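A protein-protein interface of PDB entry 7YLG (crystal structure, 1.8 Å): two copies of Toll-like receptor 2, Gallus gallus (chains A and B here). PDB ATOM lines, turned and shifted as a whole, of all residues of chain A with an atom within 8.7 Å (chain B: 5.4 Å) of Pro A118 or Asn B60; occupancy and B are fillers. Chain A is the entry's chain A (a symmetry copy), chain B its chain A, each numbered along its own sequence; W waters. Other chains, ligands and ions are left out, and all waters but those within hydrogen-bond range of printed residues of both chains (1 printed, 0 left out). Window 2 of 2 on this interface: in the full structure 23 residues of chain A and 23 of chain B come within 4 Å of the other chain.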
ATOM      1  N   PHE A  79      -0.936 -13.603  10.568  1.00  0.00           N
ATOM      2  CA  PHE A  79      -0.440 -14.900  10.111  1.00  0.00           C
ATOM      3  C   PHE A  79       0.365 -14.763   8.820  1.00  0.00           C
ATOM      4  O   PHE A  79       1.502 -15.237   8.724  1.00  0.00           O
ATOM      5  CB  PHE A  79      -1.610 -15.871   9.895  1.00  0.00           C
ATOM      6  CG  PHE A  79      -1.164 -17.275   9.561  1.00  0.00           C
ATOM      7  CD1 PHE A  79      -0.769 -17.600   8.271  1.00  0.00           C
ATOM      8  CD2 PHE A  79      -1.105 -18.256  10.554  1.00  0.00           C
ATOM      9  CE1 PHE A  79      -0.343 -18.884   7.965  1.00  0.00           C
ATOM     10  CE2 PHE A  79      -0.660 -19.549  10.260  1.00  0.00           C
ATOM     11  CZ  PHE A  79      -0.279 -19.857   8.960  1.00  0.00           C
ATOM     12  N   VAL A  80      -0.225 -14.137   7.805  1.00  0.00           N
ATOM     13  CA  VAL A  80       0.410 -14.050   6.492  1.00  0.00           C
ATOM     14  C   VAL A  80       1.720 -13.275   6.567  1.00  0.00           C
ATOM     15  O   VAL A  80       2.669 -13.571   5.825  1.00  0.00           O
ATOM     16  CB  VAL A  80      -0.569 -13.412   5.484  1.00  0.00           C
ATOM     17  CG1 VAL A  80       0.146 -13.002   4.186  1.00  0.00           C
ATOM     18  CG2 VAL A  80      -1.728 -14.379   5.202  1.00  0.00           C
ATOM     19  N   ASN A  81       1.809 -12.289   7.461  1.00  0.00           N
ATOM     20  CA  ASN A  81       3.009 -11.449   7.506  1.00  0.00           C
ATOM     21  C   ASN A  81       4.126 -12.020   8.361  1.00  0.00           C
ATOM     22  O   ASN A  81       5.232 -11.456   8.361  1.00  0.00           O
ATOM     23  CB  ASN A  81       2.677 -10.051   8.029  1.00  0.00           C
ATOM     24  CG  ASN A  81       1.808  -9.283   7.079  1.00  0.00           C
ATOM     25  OD1 ASN A  81       1.669  -9.653   5.915  1.00  0.00           O
ATOM     26  ND2 ASN A  81       1.204  -8.217   7.562  1.00  0.00           N
ATOM     27  N   SER A  82       3.871 -13.103   9.082  1.00  0.00           N
ATOM     28  CA  SER A  82       4.855 -13.666   9.989  1.00  0.00           C
ATOM     29  C   SER A  82       5.783 -14.623   9.252  1.00  0.00           C
ATOM     30  O   SER A  82       5.337 -15.460   8.469  1.00  0.00           O
ATOM     31  CB  SER A  82       4.158 -14.395  11.138  1.00  0.00           C
ATOM     32  OG  SER A  82       5.072 -15.246  11.797  1.00  0.00           O
ATOM     33  N   CYS A  83       7.079 -14.480   9.519  1.00  0.00           N
ATOM     34  CA  CYS A  83       8.097 -15.359   8.965  1.00  0.00           C
ATOM     35  C   CYS A  83       7.827 -16.819   9.328  1.00  0.00           C
ATOM     36  O   CYS A  83       7.792 -17.706   8.462  1.00  0.00           O
ATOM     37  CB  CYS A  83       9.450 -14.879   9.508  1.00  0.00           C
ATOM     38  SG  CYS A  83      10.863 -15.679   8.878  1.00  0.00           S
ATOM     39  N   GLN A  86       4.752 -18.224   7.619  1.00  0.00           N
ATOM     40  CA  GLN A  86       5.042 -18.523   6.218  1.00  0.00           C
ATOM     41  C   GLN A  86       5.778 -19.841   6.062  1.00  0.00           C
ATOM     42  O   GLN A  86       5.548 -20.566   5.092  1.00  0.00           O
ATOM     43  CB  GLN A  86       5.850 -17.384   5.586  1.00  0.00           C
ATOM     44  CG  GLN A  86       4.980 -16.168   5.334  1.00  0.00           C
ATOM     45  CD  GLN A  86       5.740 -15.080   4.594  1.00  0.00           C
ATOM     46  OE1 GLN A  86       6.751 -15.361   3.969  1.00  0.00           O
ATOM     47  NE2 GLN A  86       5.254 -13.838   4.673  1.00  0.00           N
ATOM     48  N   TYR A  87       6.715 -20.144   6.960  1.00  0.00           N
ATOM     49  CA  TYR A  87       7.387 -21.435   6.873  1.00  0.00           C
ATOM     50  C   TYR A  87       6.397 -22.569   7.077  1.00  0.00           C
ATOM     51  O   TYR A  87       6.515 -23.627   6.449  1.00  0.00           O
ATOM     52  CB  TYR A  87       8.468 -21.549   7.927  1.00  0.00           C
ATOM     53  CG  TYR A  87       9.756 -20.899   7.514  1.00  0.00           C
ATOM     54  CD1 TYR A  87      10.370 -21.237   6.326  1.00  0.00           C
ATOM     55  CD2 TYR A  87      10.355 -19.951   8.326  1.00  0.00           C
ATOM     56  CE1 TYR A  87      11.585 -20.632   5.955  1.00  0.00           C
ATOM     57  CE2 TYR A  87      11.541 -19.351   7.960  1.00  0.00           C
ATOM     58  CZ  TYR A  87      12.143 -19.692   6.772  1.00  0.00           C
ATOM     59  OH  TYR A  87      13.349 -19.090   6.419  1.00  0.00           O
ATOM     60  N   LEU A  89       3.124 -22.436   6.462  1.00  0.00           N
ATOM     61  CA  LEU A  89       2.349 -22.490   5.223  1.00  0.00           C
ATOM     62  C   LEU A  89       3.081 -23.278   4.152  1.00  0.00           C
ATOM     63  O   LEU A  89       2.502 -24.170   3.520  1.00  0.00           O
ATOM     64  CB  LEU A  89       2.062 -21.079   4.709  1.00  0.00           C
ATOM     65  CG  LEU A  89       0.636 -20.548   4.863  1.00  0.00           C
ATOM     66  CD1 LEU A  89       0.558 -19.205   4.168  1.00  0.00           C
ATOM     67  CD2 LEU A  89      -0.392 -21.523   4.297  1.00  0.00           C
ATOM     68  N   GLU A  93       1.560 -26.630   2.331  1.00  0.00           N
ATOM     69  CA  GLU A  93       1.483 -26.607   0.875  1.00  0.00           C
ATOM     70  C   GLU A  93       2.250 -27.771   0.264  1.00  0.00           C
ATOM     71  O   GLU A  93       1.693 -28.540  -0.527  1.00  0.00           O
ATOM     72  CB  GLU A  93       2.009 -25.266   0.352  1.00  0.00           C
ATOM     73  CG  GLU A  93       2.243 -25.179  -1.161  1.00  0.00           C
ATOM     74  CD  GLU A  93       1.768 -23.854  -1.786  1.00  0.00           C
ATOM     75  OE1 GLU A  93       1.958 -23.665  -3.010  1.00  0.00           O
ATOM     76  OE2 GLU A  93       1.186 -23.016  -1.065  1.00  0.00           O
ATOM     77  N   LEU A 112      -7.703 -10.576   4.387  1.00  0.00           N
ATOM     78  CA  LEU A 112      -6.327 -10.433   3.904  1.00  0.00           C
ATOM     79  C   LEU A 112      -6.313  -9.421   2.772  1.00  0.00           C
ATOM     80  O   LEU A 112      -7.048  -9.611   1.793  1.00  0.00           O
ATOM     81  CB  LEU A 112      -5.796 -11.776   3.414  1.00  0.00           C
ATOM     82  CG  LEU A 112      -5.941 -12.962   4.370  1.00  0.00           C
ATOM     83  CD1 LEU A 112      -5.355 -14.207   3.742  1.00  0.00           C
ATOM     84  CD2 LEU A 112      -5.258 -12.642   5.672  1.00  0.00           C
ATOM     85  N   PRO A 113      -5.522  -8.351   2.846  1.00  0.00           N
ATOM     86  CA  PRO A 113      -5.451  -7.396   1.729  1.00  0.00           C
ATOM     87  C   PRO A 113      -5.110  -8.110   0.436  1.00  0.00           C
ATOM     88  O   PRO A 113      -4.372  -9.106   0.445  1.00  0.00           O
ATOM     89  CB  PRO A 113      -4.330  -6.435   2.154  1.00  0.00           C
ATOM     90  CG  PRO A 113      -4.351  -6.477   3.642  1.00  0.00           C
ATOM     91  CD  PRO A 113      -4.752  -7.903   4.015  1.00  0.00           C
ATOM     92  N   PRO A 114      -5.645  -7.651  -0.692  1.00  0.00           N
ATOM     93  CA  PRO A 114      -5.405  -8.355  -1.958  1.00  0.00           C
ATOM     94  C   PRO A 114      -3.920  -8.408  -2.280  1.00  0.00           C
ATOM     95  O   PRO A 114      -3.196  -7.426  -2.101  1.00  0.00           O
ATOM     96  CB  PRO A 114      -6.173  -7.512  -2.985  1.00  0.00           C
ATOM     97  CG  PRO A 114      -7.127  -6.668  -2.178  1.00  0.00           C
ATOM     98  CD  PRO A 114      -6.453  -6.433  -0.867  1.00  0.00           C
ATOM     99  N   ASP A 115      -3.471  -9.578  -2.749  1.00  0.00           N
ATOM    100  CA  ASP A 115      -2.081  -9.824  -3.149  1.00  0.00           C
ATOM    101  C   ASP A 115      -1.100  -9.735  -1.982  1.00  0.00           C
ATOM    102  O   ASP A 115       0.113  -9.609  -2.193  1.00  0.00           O
ATOM    103  CB  ASP A 115      -1.647  -8.872  -4.275  1.00  0.00           C
ATOM    104  CG  ASP A 115      -2.235  -9.258  -5.620  1.00  0.00           C
ATOM    105  OD1 ASP A 115      -2.199 -10.466  -5.953  1.00  0.00           O
ATOM    106  OD2 ASP A 115      -2.744  -8.365  -6.335  1.00  0.00           O
ATOM    107  N   SER A 116      -1.582  -9.790  -0.744  1.00  0.00           N
ATOM    108  CA  SER A 116      -0.684  -9.777   0.407  1.00  0.00           C
ATOM    109  C   SER A 116      -0.040 -11.132   0.660  1.00  0.00           C
ATOM    110  O   SER A 116       1.001 -11.196   1.308  1.00  0.00           O
ATOM    111  CB  SER A 116      -1.444  -9.342   1.661  1.00  0.00           C
ATOM    112  OG  SER A 116      -2.589 -10.159   1.838  1.00  0.00           O
ATOM    113  N   VAL A 117      -0.662 -12.227   0.224  1.00  0.00           N
ATOM    114  CA  VAL A 117       0.011 -13.527   0.346  1.00  0.00           C
ATOM    115  C   VAL A 117       1.150 -13.583  -0.662  1.00  0.00           C
ATOM    116  O   VAL A 117       0.917 -13.302  -1.850  1.00  0.00           O
ATOM    117  CB  VAL A 117      -0.978 -14.667   0.088  1.00  0.00           C
ATOM    118  CG1 VAL A 117      -0.218 -15.996   0.051  1.00  0.00           C
ATOM    119  CG2 VAL A 117      -2.093 -14.666   1.140  1.00  0.00           C
ATOM    120  N   PRO A 118       2.371 -13.942  -0.261  1.00  0.00           N
ATOM    121  CA  PRO A 118       3.479 -13.974  -1.226  1.00  0.00           C
ATOM    122  C   PRO A 118       3.140 -14.826  -2.447  1.00  0.00           C
ATOM    123  O   PRO A 118       2.451 -15.851  -2.355  1.00  0.00           O
ATOM    124  CB  PRO A 118       4.640 -14.558  -0.411  1.00  0.00           C
ATOM    125  CG  PRO A 118       4.335 -14.142   1.003  1.00  0.00           C
ATOM    126  CD  PRO A 118       2.820 -14.280   1.104  1.00  0.00           C
ATOM    127  N   GLN A 119       3.623 -14.372  -3.609  1.00  0.00           N
ATOM    128  CA  GLN A 119       3.177 -14.942  -4.875  1.00  0.00           C
ATOM    129  C   GLN A 119       3.565 -16.410  -4.994  1.00  0.00           C
ATOM    130  O   GLN A 119       2.854 -17.186  -5.640  1.00  0.00           O
ATOM    131  CB  GLN A 119       3.730 -14.128  -6.044  1.00  0.00           C
ATOM    132  CG  GLN A 119       3.289 -12.657  -6.047  1.00  0.00           C
ATOM    133  CD  GLN A 119       1.835 -12.465  -6.478  1.00  0.00           C
ATOM    134  OE1 GLN A 119       1.394 -13.030  -7.477  1.00  0.00           O
ATOM    135  NE2 GLN A 119       1.087 -11.671  -5.718  1.00  0.00           N
ATOM    136  N   LYS A 120       4.641 -16.827  -4.327  1.00  0.00           N
ATOM    137  CA  LYS A 120       5.068 -18.215  -4.441  1.00  0.00           C
ATOM    138  C   LYS A 120       4.221 -19.202  -3.638  1.00  0.00           C
ATOM    139  O   LYS A 120       4.443 -20.407  -3.773  1.00  0.00           O
ATOM    140  CB  LYS A 120       6.528 -18.337  -4.031  1.00  0.00           C
ATOM    141  CG  LYS A 120       7.423 -17.421  -4.814  1.00  0.00           C
ATOM    142  CD  LYS A 120       8.487 -18.205  -5.533  1.00  0.00           C
ATOM    143  CE  LYS A 120       9.195 -17.332  -6.542  1.00  0.00           C
ATOM    144  NZ  LYS A 120      10.219 -18.127  -7.246  1.00  0.00           N
ATOM    145  N   PHE A 121       3.277 -18.743  -2.813  1.00  0.00           N
ATOM    146  CA  PHE A 121       2.305 -19.640  -2.170  1.00  0.00           C
ATOM    147  C   PHE A 121       1.117 -19.857  -3.112  1.00  0.00           C
ATOM    148  O   PHE A 121      -0.015 -19.476  -2.826  1.00  0.00           O
ATOM    149  CB  PHE A 121       1.842 -19.075  -0.832  1.00  0.00           C
ATOM    150  CG  PHE A 121       2.906 -19.058   0.231  1.00  0.00           C
ATOM    151  CD1 PHE A 121       3.634 -20.191   0.523  1.00  0.00           C
ATOM    152  CD2 PHE A 121       3.191 -17.894   0.923  1.00  0.00           C
ATOM    153  CE1 PHE A 121       4.631 -20.171   1.499  1.00  0.00           C
ATOM    154  CE2 PHE A 121       4.183 -17.867   1.896  1.00  0.00           C
ATOM    155  CZ  PHE A 121       4.901 -19.011   2.185  1.00  0.00           C
ATOM    156  N   SER A 122       1.409 -20.449  -4.270  1.00  0.00           N
ATOM    157  CA  SER A 122       0.443 -20.418  -5.366  1.00  0.00           C
ATOM    158  C   SER A 122      -0.780 -21.282  -5.080  1.00  0.00           C
ATOM    159  O   SER A 122      -1.881 -20.958  -5.538  1.00  0.00           O
ATOM    160  CB  SER A 122       1.112 -20.849  -6.668  1.00  0.00           C
ATOM    161  OG  SER A 122       1.867 -22.026  -6.470  1.00  0.00           O
ATOM    162  N   LYS A 123      -0.613 -22.365  -4.318  1.00  0.00           N
ATOM    163  CA  LYS A 123      -1.755 -23.200  -3.961  1.00  0.00           C
ATOM    164  C   LYS A 123      -2.676 -22.472  -2.996  1.00  0.00           C
ATOM    165  O   LYS A 123      -3.885 -22.375  -3.234  1.00  0.00           O
ATOM    166  CB  LYS A 123      -1.275 -24.521  -3.362  1.00  0.00           C
ATOM    167  N   LEU A 124      -2.122 -21.947  -1.899  1.00  0.00           N
ATOM    168  CA  LEU A 124      -2.922 -21.135  -0.990  1.00  0.00           C
ATOM    169  C   LEU A 124      -3.570 -19.968  -1.723  1.00  0.00           C
ATOM    170  O   LEU A 124      -4.730 -19.633  -1.461  1.00  0.00           O
ATOM    171  CB  LEU A 124      -2.064 -20.625   0.166  1.00  0.00           C
ATOM    172  N   ARG A 125      -2.829 -19.332  -2.647  1.00  0.00           N
ATOM    173  CA  ARG A 125      -3.392 -18.211  -3.392  1.00  0.00           C
ATOM    174  C   ARG A 125      -4.577 -18.651  -4.255  1.00  0.00           C
ATOM    175  O   ARG A 125      -5.598 -17.957  -4.316  1.00  0.00           O
ATOM    176  CB  ARG A 125      -2.302 -17.554  -4.243  1.00  0.00           C
ATOM    177  CG  ARG A 125      -1.357 -16.714  -3.378  1.00  0.00           C
ATOM    178  CD  ARG A 125      -0.286 -15.981  -4.204  1.00  0.00           C
ATOM    179  NE  ARG A 125      -0.826 -15.359  -5.410  1.00  0.00           N
ATOM    180  CZ  ARG A 125      -0.514 -15.735  -6.646  1.00  0.00           C
ATOM    181  NH1 ARG A 125       0.349 -16.724  -6.851  1.00  0.00           N
ATOM    182  NH2 ARG A 125      -1.059 -15.117  -7.684  1.00  0.00           N
ATOM    183  N   LYS A 126      -4.463 -19.799  -4.924  1.00  0.00           N
ATOM    184  CA  LYS A 126      -5.595 -20.295  -5.717  1.00  0.00           C
ATOM    185  C   LYS A 126      -6.801 -20.608  -4.834  1.00  0.00           C
ATOM    186  O   LYS A 126      -7.948 -20.307  -5.202  1.00  0.00           O
ATOM    187  CB  LYS A 126      -5.171 -21.524  -6.519  1.00  0.00           C
ATOM    188  CG  LYS A 126      -4.266 -21.217  -7.723  1.00  0.00           C
ATOM    189  N   LEU A 128      -7.667 -19.170  -2.027  1.00  0.00           N
ATOM    190  CA  LEU A 128      -8.326 -17.928  -1.630  1.00  0.00           C
ATOM    191  C   LEU A 128      -9.047 -17.286  -2.805  1.00  0.00           C
ATOM    192  O   LEU A 128     -10.166 -16.774  -2.653  1.00  0.00           O
ATOM    193  CB  LEU A 128      -7.302 -16.954  -1.027  1.00  0.00           C
ATOM    194  CG  LEU A 128      -6.690 -17.332   0.319  1.00  0.00           C
ATOM    195  CD1 LEU A 128      -5.364 -16.541   0.574  1.00  0.00           C
ATOM    196  CD2 LEU A 128      -7.729 -17.072   1.432  1.00  0.00           C
ATOM    197  N   HIS B  47      16.835 -13.155   8.884  1.00  0.00           N
ATOM    198  CA  HIS B  47      15.474 -12.653   9.043  1.00  0.00           C
ATOM    199  C   HIS B  47      15.346 -11.681  10.207  1.00  0.00           C
ATOM    200  O   HIS B  47      14.578 -10.717  10.128  1.00  0.00           O
ATOM    201  CB  HIS B  47      14.503 -13.832   9.219  1.00  0.00           C
ATOM    202  CG  HIS B  47      14.252 -14.592   7.954  1.00  0.00           C
ATOM    203  ND1 HIS B  47      14.367 -14.021   6.702  1.00  0.00           N
ATOM    204  CD2 HIS B  47      13.871 -15.875   7.747  1.00  0.00           C
ATOM    205  CE1 HIS B  47      14.079 -14.922   5.779  1.00  0.00           C
ATOM    206  NE2 HIS B  47      13.774 -16.056   6.388  1.00  0.00           N
ATOM    207  N   PHE B  51      14.098  -9.356   7.557  1.00  0.00           N
ATOM    208  CA  PHE B  51      12.691  -9.627   7.282  1.00  0.00           C
ATOM    209  C   PHE B  51      11.859  -8.473   7.820  1.00  0.00           C
ATOM    210  O   PHE B  51      11.949  -8.124   8.999  1.00  0.00           O
ATOM    211  CB  PHE B  51      12.259 -10.955   7.919  1.00  0.00           C
ATOM    212  CG  PHE B  51      10.876 -11.419   7.526  1.00  0.00           C
ATOM    213  CD1 PHE B  51       9.755 -10.974   8.213  1.00  0.00           C
ATOM    214  CD2 PHE B  51      10.698 -12.327   6.496  1.00  0.00           C
ATOM    215  CE1 PHE B  51       8.458 -11.422   7.873  1.00  0.00           C
ATOM    216  CE2 PHE B  51       9.415 -12.789   6.156  1.00  0.00           C
ATOM    217  CZ  PHE B  51       8.293 -12.325   6.844  1.00  0.00           C
ATOM    218  N   HIS B  55       6.153  -6.017   4.148  1.00  0.00           N
ATOM    219  CA  HIS B  55       6.837  -5.476   2.988  1.00  0.00           C
ATOM    220  C   HIS B  55       6.671  -6.461   1.837  1.00  0.00           C
ATOM    221  O   HIS B  55       6.881  -7.668   2.026  1.00  0.00           O
ATOM    222  CB  HIS B  55       8.317  -5.234   3.314  1.00  0.00           C
ATOM    223  CG  HIS B  55       9.032  -4.403   2.299  1.00  0.00           C
ATOM    224  ND1 HIS B  55       9.296  -4.851   1.024  1.00  0.00           N
ATOM    225  CD2 HIS B  55       9.548  -3.151   2.374  1.00  0.00           C
ATOM    226  CE1 HIS B  55       9.949  -3.912   0.357  1.00  0.00           C
ATOM    227  NE2 HIS B  55      10.110  -2.867   1.152  1.00  0.00           N
ATOM    228  N   PRO B  56       6.237  -6.007   0.660  1.00  0.00           N
ATOM    229  CA  PRO B  56       5.968  -6.956  -0.430  1.00  0.00           C
ATOM    230  C   PRO B  56       7.205  -7.662  -0.956  1.00  0.00           C
ATOM    231  O   PRO B  56       7.080  -8.770  -1.486  1.00  0.00           O
ATOM    232  CB  PRO B  56       5.314  -6.075  -1.501  1.00  0.00           C
ATOM    233  CG  PRO B  56       5.897  -4.669  -1.227  1.00  0.00           C
ATOM    234  CD  PRO B  56       5.939  -4.614   0.277  1.00  0.00           C
ATOM    235  N   VAL B  57       8.397  -7.082  -0.824  1.00  0.00           N
ATOM    236  CA  VAL B  57       9.627  -7.751  -1.219  1.00  0.00           C
ATOM    237  C   VAL B  57      10.324  -8.391  -0.032  1.00  0.00           C
ATOM    238  O   VAL B  57      10.725  -9.549  -0.092  1.00  0.00           O
ATOM    239  CB  VAL B  57      10.569  -6.758  -1.936  1.00  0.00           C
ATOM    240  CG1 VAL B  57      11.903  -7.453  -2.264  1.00  0.00           C
ATOM    241  CG2 VAL B  57       9.893  -6.242  -3.175  1.00  0.00           C
ATOM    242  N   LEU B  58      10.478  -7.647   1.059  1.00  0.00           N
ATOM    243  CA  LEU B  58      11.307  -8.089   2.172  1.00  0.00           C
ATOM    244  C   LEU B  58      10.506  -8.825   3.224  1.00  0.00           C
ATOM    245  O   LEU B  58      11.091  -9.319   4.196  1.00  0.00           O
ATOM    246  CB  LEU B  58      12.016  -6.881   2.804  1.00  0.00           C
ATOM    247  CG  LEU B  58      12.900  -6.075   1.853  1.00  0.00           C
ATOM    248  CD1 LEU B  58      13.321  -4.769   2.525  1.00  0.00           C
ATOM    249  CD2 LEU B  58      14.107  -6.879   1.432  1.00  0.00           C
ATOM    250  N   GLY B  59       9.200  -8.941   3.032  1.00  0.00           N
ATOM    251  CA  GLY B  59       8.342  -9.538   4.033  1.00  0.00           C
ATOM    252  C   GLY B  59       7.877 -10.914   3.628  1.00  0.00           C
ATOM    253  O   GLY B  59       6.768 -11.337   3.996  1.00  0.00           O
ATOM    254  N   ASN B  60       8.720 -11.649   2.900  1.00  0.00           N
ATOM    255  CA  ASN B  60       8.424 -13.054   2.688  1.00  0.00           C
ATOM    256  C   ASN B  60       9.696 -13.890   2.701  1.00  0.00           C
ATOM    257  O   ASN B  60      10.809 -13.396   2.457  1.00  0.00           O
ATOM    258  CB  ASN B  60       7.636 -13.269   1.406  1.00  0.00           C
ATOM    259  CG  ASN B  60       8.426 -12.958   0.194  1.00  0.00           C
ATOM    260  OD1 ASN B  60       9.176 -13.786  -0.279  1.00  0.00           O
ATOM    261  ND2 ASN B  60       8.235 -11.776  -0.347  1.00  0.00           N
ATOM    262  N   ILE B  61       9.508 -15.173   3.012  1.00  0.00           N
ATOM    263  CA  ILE B  61      10.628 -16.068   3.283  1.00  0.00           C
ATOM    264  C   ILE B  61      11.410 -16.423   2.035  1.00  0.00           C
ATOM    265  O   ILE B  61      12.490 -17.010   2.146  1.00  0.00           O
ATOM    266  CB  ILE B  61      10.155 -17.376   3.944  1.00  0.00           C
ATOM    267  CG1 ILE B  61       9.092 -18.044   3.071  1.00  0.00           C
ATOM    268  CG2 ILE B  61       9.605 -17.112   5.353  1.00  0.00           C
ATOM    269  CD1 ILE B  61       8.747 -19.491   3.515  1.00  0.00           C
ATOM    270  N   PHE B  62      10.898 -16.104   0.848  1.00  0.00           N
ATOM    271  CA  PHE B  62      11.655 -16.452  -0.347  1.00  0.00           C
ATOM    272  C   PHE B  62      12.767 -15.449  -0.635  1.00  0.00           C
ATOM    273  O   PHE B  62      13.740 -15.805  -1.306  1.00  0.00           O
ATOM    274  CB  PHE B  62      10.718 -16.561  -1.543  1.00  0.00           C
ATOM    275  CG  PHE B  62       9.652 -17.610  -1.365  1.00  0.00           C
ATOM    276  CD1 PHE B  62       9.893 -18.913  -1.732  1.00  0.00           C
ATOM    277  CD2 PHE B  62       8.424 -17.285  -0.806  1.00  0.00           C
ATOM    278  CE1 PHE B  62       8.902 -19.900  -1.557  1.00  0.00           C
ATOM    279  CE2 PHE B  62       7.441 -18.249  -0.618  1.00  0.00           C
ATOM    280  CZ  PHE B  62       7.679 -19.552  -1.000  1.00  0.00           C
ATOM    281  N   TYR B  63      12.655 -14.231  -0.111  1.00  0.00           N
ATOM    282  CA  TYR B  63      13.578 -13.156  -0.495  1.00  0.00           C
ATOM    283  C   TYR B  63      15.033 -13.515  -0.197  1.00  0.00           C
ATOM    284  O   TYR B  63      15.904 -13.396  -1.071  1.00  0.00           O
ATOM    285  CB  TYR B  63      13.197 -11.868   0.229  1.00  0.00           C
ATOM    286  CG  TYR B  63      14.246 -10.796   0.023  1.00  0.00           C
ATOM    287  CD1 TYR B  63      14.272 -10.058  -1.145  1.00  0.00           C
ATOM    288  CD2 TYR B  63      15.229 -10.562   0.982  1.00  0.00           C
ATOM    289  CE1 TYR B  63      15.256  -9.071  -1.360  1.00  0.00           C
ATOM    290  CE2 TYR B  63      16.236  -9.586   0.776  1.00  0.00           C
ATOM    291  CZ  TYR B  63      16.228  -8.849  -0.395  1.00  0.00           C
ATOM    292  OH  TYR B  63      17.200  -7.887  -0.627  1.00  0.00           O
ATOM    293  N   CYS B  64      15.336 -13.907   1.044  1.00  0.00           N
ATOM    294  CA  CYS B  64      16.748 -14.065   1.411  1.00  0.00           C
ATOM    295  C   CYS B  64      17.382 -15.219   0.647  1.00  0.00           C
ATOM    296  O   CYS B  64      18.456 -15.074   0.044  1.00  0.00           O
ATOM    297  CB  CYS B  64      16.901 -14.271   2.919  1.00  0.00           C
ATOM    298  SG  CYS B  64      16.894 -12.771   3.928  1.00  0.00           S
HETATM  299  O   HOH W   1       5.279 -10.090   5.606  1.00  0.00           O
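A ring nitrogen (NE2) of His B47 sits at hydrogen-bond distance from the side-chain hydroxyl of Tyr A87 (3.1 Å). The backbone carbonyl oxygen (O) of Gly B59 lies within hydrogen-bond range of the side-chain amide nitrogen (NE2) of Gln A86, at 3.0 Å. N of Ile B61 sits at hydrogen-bond distance from OE1 of Gln A86 (2.9 Å).
ND2 of Asn B60 is in hydrogen-bond range of O of Pro B56 (3.4 Å). The backbone carbonyl oxygen (O) of Val B57 is in hydrogen-bond range of the side-chain amide nitrogen (ND2) of Asn B60 (3.4 Å). N of Phe B62 is in hydrogen-bond range of OD1 of Asn B60. The backbone carbonyl oxygen of Val A80 sits at hydrogen-bond distance from the side-chain amide nitrogen of Gln A86, at 2.8 Å.
Among the printed residues, merely in contact across the chains: Asn A81 with Phe B51, Cys A83 with His B47, Cys A83 with Phe B51, Cys A83 with Ile B61, Gln A86 with Asn B60, Tyr A87 with Ile B61, Pro A118 with Asn B60, Lys A120 with Phe B62 and Phe A121 with Phe B62.
Of the printed residues of chain A, Asn B60 touches Gln A86 (3.1 Å) and Pro A118 (3.4 Å). Of chain A, only Gln A86 (3.0 Å) comes within 4 Å of Gly B59. Of the printed residues of chain B, Asn A81 touches Phe B51. Of the printed residues of chain B, Lys A120 touches Phe B62. The nearest residue of chain B that does not touch Pro A118 is Phe B62 (4.6 Å). The nearest printed residue of chain A that does not touch Ile B61 is Phe A121 (4.1 Å).
Of the 12 printed residues of chain B, 6 touch a printed residue of chain A. Hydrophobic or aromatic side chains of chain B within 4 Å of the printed part of chain A: His B47, Phe B51, Ile B61 and Phe B62. Among the printed residues, 12 pairs touch across the chains.
No position is printed for both chains.
Water W1 bridges O of Gly B59 (2.5 Å) and O of Asn A81 (3.1 Å).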
